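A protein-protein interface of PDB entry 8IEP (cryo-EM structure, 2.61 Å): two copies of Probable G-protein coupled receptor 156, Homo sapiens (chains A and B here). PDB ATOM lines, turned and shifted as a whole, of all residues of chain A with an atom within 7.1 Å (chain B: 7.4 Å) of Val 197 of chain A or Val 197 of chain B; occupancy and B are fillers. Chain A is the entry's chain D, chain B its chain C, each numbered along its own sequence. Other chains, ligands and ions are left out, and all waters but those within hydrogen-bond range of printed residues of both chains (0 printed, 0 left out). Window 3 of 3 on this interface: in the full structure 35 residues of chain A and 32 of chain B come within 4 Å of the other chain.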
ATOM      1  N   LEU A 195     -15.443 -17.316 -15.084  1.00  0.00           N
ATOM      2  CA  LEU A 195     -16.427 -17.362 -16.157  1.00  0.00           C
ATOM      3  C   LEU A 195     -17.235 -16.077 -16.095  1.00  0.00           C
ATOM      4  O   LEU A 195     -17.636 -15.645 -15.009  1.00  0.00           O
ATOM      5  CB  LEU A 195     -17.325 -18.602 -16.039  1.00  0.00           C
ATOM      6  CG  LEU A 195     -18.206 -18.796 -14.798  1.00  0.00           C
ATOM      7  CD1 LEU A 195     -19.583 -18.139 -14.940  1.00  0.00           C
ATOM      8  CD2 LEU A 195     -18.356 -20.279 -14.491  1.00  0.00           C
ATOM      9  N   SER A 196     -17.430 -15.444 -17.248  1.00  0.00           N
ATOM     10  CA  SER A 196     -18.088 -14.147 -17.288  1.00  0.00           C
ATOM     11  C   SER A 196     -18.706 -13.926 -18.658  1.00  0.00           C
ATOM     12  O   SER A 196     -18.235 -14.474 -19.658  1.00  0.00           O
ATOM     13  CB  SER A 196     -17.100 -13.019 -16.970  1.00  0.00           C
ATOM     14  OG  SER A 196     -16.362 -12.648 -18.121  1.00  0.00           O
ATOM     15  N   VAL A 197     -19.765 -13.120 -18.686  1.00  0.00           N
ATOM     16  CA  VAL A 197     -20.425 -12.695 -19.914  1.00  0.00           C
ATOM     17  C   VAL A 197     -20.415 -11.174 -19.943  1.00  0.00           C
ATOM     18  O   VAL A 197     -20.797 -10.528 -18.959  1.00  0.00           O
ATOM     19  CB  VAL A 197     -21.861 -13.246 -20.019  1.00  0.00           C
ATOM     20  CG1 VAL A 197     -21.833 -14.741 -20.281  1.00  0.00           C
ATOM     21  CG2 VAL A 197     -22.676 -12.941 -18.758  1.00  0.00           C
ATOM     22  N   SER A 198     -19.967 -10.608 -21.061  1.00  0.00           N
ATOM     23  CA  SER A 198     -19.790  -9.170 -21.212  1.00  0.00           C
ATOM     24  C   SER A 198     -20.659  -8.668 -22.353  1.00  0.00           C
ATOM     25  O   SER A 198     -20.643  -9.241 -23.448  1.00  0.00           O
ATOM     26  CB  SER A 198     -18.321  -8.826 -21.478  1.00  0.00           C
ATOM     27  OG  SER A 198     -17.486  -9.328 -20.449  1.00  0.00           O
ATOM     28  N   MET A 199     -21.408  -7.597 -22.096  1.00  0.00           N
ATOM     29  CA  MET A 199     -22.264  -6.964 -23.099  1.00  0.00           C
ATOM     30  C   MET A 199     -21.507  -5.762 -23.655  1.00  0.00           C
ATOM     31  O   MET A 199     -21.678  -4.631 -23.200  1.00  0.00           O
ATOM     32  CB  MET A 199     -23.602  -6.556 -22.494  1.00  0.00           C
ATOM     33  CG  MET A 199     -24.485  -7.730 -22.101  1.00  0.00           C
ATOM     34  SD  MET A 199     -26.087  -7.212 -21.457  1.00  0.00           S
ATOM     35  CE  MET A 199     -26.906  -6.685 -22.961  1.00  0.00           C
ATOM     36  N   THR A 200     -20.664  -6.016 -24.650  1.00  0.00           N
ATOM     37  CA  THR A 200     -19.870  -4.960 -25.270  1.00  0.00           C
ATOM     38  C   THR A 200     -20.768  -4.115 -26.164  1.00  0.00           C
ATOM     39  O   THR A 200     -21.337  -4.620 -27.137  1.00  0.00           O
ATOM     40  CB  THR A 200     -18.721  -5.565 -26.072  1.00  0.00           C
ATOM     41  OG1 THR A 200     -17.933  -6.408 -25.223  1.00  0.00           O
ATOM     42  CG2 THR A 200     -17.839  -4.475 -26.662  1.00  0.00           C
ATOM     43  N   CYS A 208     -22.741  -9.358 -27.359  1.00  0.00           N
ATOM     44  CA  CYS A 208     -22.536 -10.095 -26.121  1.00  0.00           C
ATOM     45  C   CYS A 208     -21.599 -11.264 -26.384  1.00  0.00           C
ATOM     46  O   CYS A 208     -21.647 -11.879 -27.453  1.00  0.00           O
ATOM     47  CB  CYS A 208     -23.863 -10.604 -25.549  1.00  0.00           C
ATOM     48  SG  CYS A 208     -23.703 -11.512 -23.993  1.00  0.00           S
ATOM     49  N   THR A 209     -20.746 -11.560 -25.405  1.00  0.00           N
ATOM     50  CA  THR A 209     -19.765 -12.628 -25.505  1.00  0.00           C
ATOM     51  C   THR A 209     -19.791 -13.465 -24.233  1.00  0.00           C
ATOM     52  O   THR A 209     -20.153 -12.984 -23.157  1.00  0.00           O
ATOM     53  CB  THR A 209     -18.350 -12.076 -25.730  1.00  0.00           C
ATOM     54  OG1 THR A 209     -18.067 -11.063 -24.756  1.00  0.00           O
ATOM     55  CG2 THR A 209     -18.221 -11.485 -27.124  1.00  0.00           C
ATOM     56  N   SER A 210     -19.402 -14.731 -24.377  1.00  0.00           N
ATOM     57  CA  SER A 210     -19.319 -15.675 -23.266  1.00  0.00           C
ATOM     58  C   SER A 210     -17.891 -16.194 -23.198  1.00  0.00           C
ATOM     59  O   SER A 210     -17.437 -16.891 -24.113  1.00  0.00           O
ATOM     60  CB  SER A 210     -20.311 -16.825 -23.441  1.00  0.00           C
ATOM     61  OG  SER A 210     -21.641 -16.390 -23.221  1.00  0.00           O
ATOM     62  N   THR A 211     -17.188 -15.856 -22.119  1.00  0.00           N
ATOM     63  CA  THR A 211     -15.784 -16.203 -21.939  1.00  0.00           C
ATOM     64  C   THR A 211     -15.605 -16.938 -20.619  1.00  0.00           C
ATOM     65  O   THR A 211     -16.105 -16.490 -19.582  1.00  0.00           O
ATOM     66  CB  THR A 211     -14.901 -14.953 -21.965  1.00  0.00           C
ATOM     67  OG1 THR A 211     -15.335 -14.036 -20.953  1.00  0.00           O
ATOM     68  CG2 THR A 211     -14.973 -14.275 -23.325  1.00  0.00           C
ATOM     69  N   ILE B 194     -18.141  -1.422 -21.271  1.00  0.00           N
ATOM     70  CA  ILE B 194     -18.135  -2.841 -20.936  1.00  0.00           C
ATOM     71  C   ILE B 194     -18.848  -3.021 -19.605  1.00  0.00           C
ATOM     72  O   ILE B 194     -18.417  -2.474 -18.582  1.00  0.00           O
ATOM     73  CB  ILE B 194     -16.706  -3.402 -20.868  1.00  0.00           C
ATOM     74  CG1 ILE B 194     -16.020  -3.333 -22.240  1.00  0.00           C
ATOM     75  CG2 ILE B 194     -16.716  -4.829 -20.326  1.00  0.00           C
ATOM     76  CD1 ILE B 194     -16.612  -4.239 -23.315  1.00  0.00           C
ATOM     77  N   LEU B 195     -19.938  -3.785 -19.622  1.00  0.00           N
ATOM     78  CA  LEU B 195     -20.614  -4.241 -18.415  1.00  0.00           C
ATOM     79  C   LEU B 195     -20.658  -5.759 -18.455  1.00  0.00           C
ATOM     80  O   LEU B 195     -20.972  -6.348 -19.494  1.00  0.00           O
ATOM     81  CB  LEU B 195     -22.022  -3.640 -18.301  1.00  0.00           C
ATOM     82  CG  LEU B 195     -23.086  -3.978 -19.353  1.00  0.00           C
ATOM     83  CD1 LEU B 195     -23.884  -5.238 -19.006  1.00  0.00           C
ATOM     84  CD2 LEU B 195     -24.024  -2.794 -19.541  1.00  0.00           C
ATOM     85  N   SER B 196     -20.308  -6.390 -17.337  1.00  0.00           N
ATOM     86  CA  SER B 196     -20.189  -7.839 -17.298  1.00  0.00           C
ATOM     87  C   SER B 196     -20.366  -8.327 -15.870  1.00  0.00           C
ATOM     88  O   SER B 196     -20.205  -7.566 -14.911  1.00  0.00           O
ATOM     89  CB  SER B 196     -18.832  -8.299 -17.844  1.00  0.00           C
ATOM     90  OG  SER B 196     -17.778  -7.893 -16.989  1.00  0.00           O
ATOM     91  N   VAL B 197     -20.699  -9.608 -15.747  1.00  0.00           N
ATOM     92  CA  VAL B 197     -20.786 -10.298 -14.466  1.00  0.00           C
ATOM     93  C   VAL B 197     -19.783 -11.442 -14.495  1.00  0.00           C
ATOM     94  O   VAL B 197     -19.786 -12.251 -15.428  1.00  0.00           O
ATOM     95  CB  VAL B 197     -22.213 -10.812 -14.181  1.00  0.00           C
ATOM     96  CG1 VAL B 197     -23.135  -9.648 -13.859  1.00  0.00           C
ATOM     97  CG2 VAL B 197     -22.772 -11.621 -15.358  1.00  0.00           C
ATOM     98  N   SER B 198     -18.918 -11.496 -13.484  1.00  0.00           N
ATOM     99  CA  SER B 198     -17.818 -12.450 -13.433  1.00  0.00           C
ATOM    100  C   SER B 198     -17.935 -13.294 -12.176  1.00  0.00           C
ATOM    101  O   SER B 198     -18.100 -12.758 -11.076  1.00  0.00           O
ATOM    102  CB  SER B 198     -16.466 -11.731 -13.459  1.00  0.00           C
ATOM    103  OG  SER B 198     -16.246 -11.020 -12.254  1.00  0.00           O
ATOM    104  N   MET B 199     -17.847 -14.612 -12.344  1.00  0.00           N
ATOM    105  CA  MET B 199     -17.874 -15.571 -11.245  1.00  0.00           C
ATOM    106  C   MET B 199     -16.474 -16.155 -11.108  1.00  0.00           C
ATOM    107  O   MET B 199     -16.011 -16.883 -11.992  1.00  0.00           O
ATOM    108  CB  MET B 199     -18.912 -16.662 -11.504  1.00  0.00           C
ATOM    109  CG  MET B 199     -19.046 -17.685 -10.388  1.00  0.00           C
ATOM    110  SD  MET B 199     -20.367 -18.868 -10.710  1.00  0.00           S
ATOM    111  CE  MET B 199     -20.169 -19.987  -9.327  1.00  0.00           C
ATOM    112  N   CYS B 208     -18.399 -13.496  -6.656  1.00  0.00           N
ATOM    113  CA  CYS B 208     -19.087 -12.907  -7.796  1.00  0.00           C
ATOM    114  C   CYS B 208     -18.990 -11.393  -7.709  1.00  0.00           C
ATOM    115  O   CYS B 208     -19.113 -10.816  -6.624  1.00  0.00           O
ATOM    116  CB  CYS B 208     -20.559 -13.334  -7.840  1.00  0.00           C
ATOM    117  SG  CYS B 208     -20.815 -15.080  -8.230  1.00  0.00           S
ATOM    118  N   THR B 209     -18.761 -10.755  -8.854  1.00  0.00           N
ATOM    119  CA  THR B 209     -18.651  -9.307  -8.930  1.00  0.00           C
ATOM    120  C   THR B 209     -19.232  -8.827 -10.250  1.00  0.00           C
ATOM    121  O   THR B 209     -19.090  -9.495 -11.279  1.00  0.00           O
ATOM    122  CB  THR B 209     -17.192  -8.845  -8.805  1.00  0.00           C
ATOM    123  OG1 THR B 209     -16.556  -9.546  -7.730  1.00  0.00           O
ATOM    124  CG2 THR B 209     -17.120  -7.347  -8.543  1.00  0.00           C
ATOM    125  N   SER B 210     -19.892  -7.672 -10.209  1.00  0.00           N
ATOM    126  CA  SER B 210     -20.469  -7.030 -11.385  1.00  0.00           C
ATOM    127  C   SER B 210     -19.810  -5.666 -11.537  1.00  0.00           C
ATOM    128  O   SER B 210     -19.868  -4.841 -10.620  1.00  0.00           O
ATOM    129  CB  SER B 210     -21.985  -6.899 -11.249  1.00  0.00           C
ATOM    130  OG  SER B 210     -22.564  -8.125 -10.838  1.00  0.00           O
ATOM    131  N   THR B 211     -19.181  -5.435 -12.687  1.00  0.00           N
ATOM    132  CA  THR B 211     -18.445  -4.208 -12.960  1.00  0.00           C
ATOM    133  C   THR B 211     -18.886  -3.637 -14.298  1.00  0.00           C
ATOM    134  O   THR B 211     -18.991  -4.369 -15.287  1.00  0.00           O
ATOM    135  CB  THR B 211     -16.935  -4.464 -12.974  1.00  0.00           C
ATOM    136  OG1 THR B 211     -16.620  -5.429 -13.986  1.00  0.00           O
ATOM    137  CG2 THR B 211     -16.463  -4.977 -11.621  1.00  0.00           C
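O of Leu 195 of chain B sits at hydrogen-bond distance from N of Met 199 of chain A, 2.9 Å away.
The backbone NH (N) of Val 197 of chain B is in hydrogen-bond range of the backbone carbonyl oxygen (O) of Val 197 of chain A, at 3.3 Å.
N of Met 199 of chain B sits at hydrogen-bond distance from O of Leu 195 of chain A, 2.9 Å away.
N of Ser 196 of chain B lies within hydrogen-bond range of O of Thr 211 of chain B (3.2 Å).
The backbone NH (N) of Ser 198 of chain B sits at hydrogen-bond distance from the backbone carbonyl oxygen (O) of Thr 209 of chain B, 3.0 Å away.
O of Thr 211 of chain A is in hydrogen-bond range of N of Ser 196 of chain A, at 2.9 Å.
O of Ser 198 of chain A sits at hydrogen-bond distance from N of Thr 209 of chain A.
Ser 198 of chain B touches Leu 195 of chain A.
Ser 196 of chain A touches Val 197 of chain B (CA to O, 3.2 Å).
Ser 198 of chain B touches Ser 196 of chain A.
O of Val 197 of chain A touches CB of Ser 196 of chain B, at 3.2 Å.
Ser 198 of chain A touches Leu 195 of chain B.
Ser 198 of chain A touches Ser 196 of chain B (OG to CB, 3.1 Å).
CD1 of Ile 194 of chain B touches OG1 of Thr 200 of chain A, 3.2 Å away.
Of the printed residues of chain B, Val 197 of chain A touches Ser 196 (3.2 Å) and Val 197 (3.3 Å).
Val 197 of chain B touches two residues of chain A.
Of the printed residues of chain B, Ser 196 of chain A touches Val 197 and Ser 198.
Printed residues of chain A within 4 Å of Ile 194 of chain B: Thr 200 (3.2 Å).
Printed residues of chain A within 4 Å of Met 199 of chain B: Leu 195.
Printed residues of chain A within 4 Å of Ser 198 of chain B: Leu 195 and Ser 196.
Cys 208 of chain A touches none of the printed residues of chain B.
The nearest residue of chain A that does not touch Val 197 of chain B is Leu 195 of chain A (4.04 Å).
The nearest printed residue of chain A that does not touch Ser 196 of chain B is Met 199 of chain A (5.0 Å).
Of the 10 printed residues of chain B, 6 touch a printed residue of chain A.
Hydrophobic or aromatic side chains of chain B within 4 Å of the printed part of chain A: Ile 194, Leu 195, Val 197 and Met 199.
Of the 10 printed residues of chain A, 6 touch a printed residue of chain B.
Printed residues of chain A that touch a printed residue of chain B: Leu 195, Ser 196, Val 197, Ser 198, Met 199 and Thr 200.
Leu 195 of chain A touches Ser 198 of chain B, and with the chains exchanged Ser 198 of chain A touches Leu 195 of chain B.
Leu 195 of chain A touches Met 199 of chain B, and with the chains exchanged Met 199 of chain A touches Leu 195 of chain B.
Ser 196 of chain A touches Ser 198 of chain B, and with the chains exchanged Ser 198 of chain A touches Ser 196 of chain B.
Val 197 of chain B touches its own counterpart, Val 197 of chain A.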
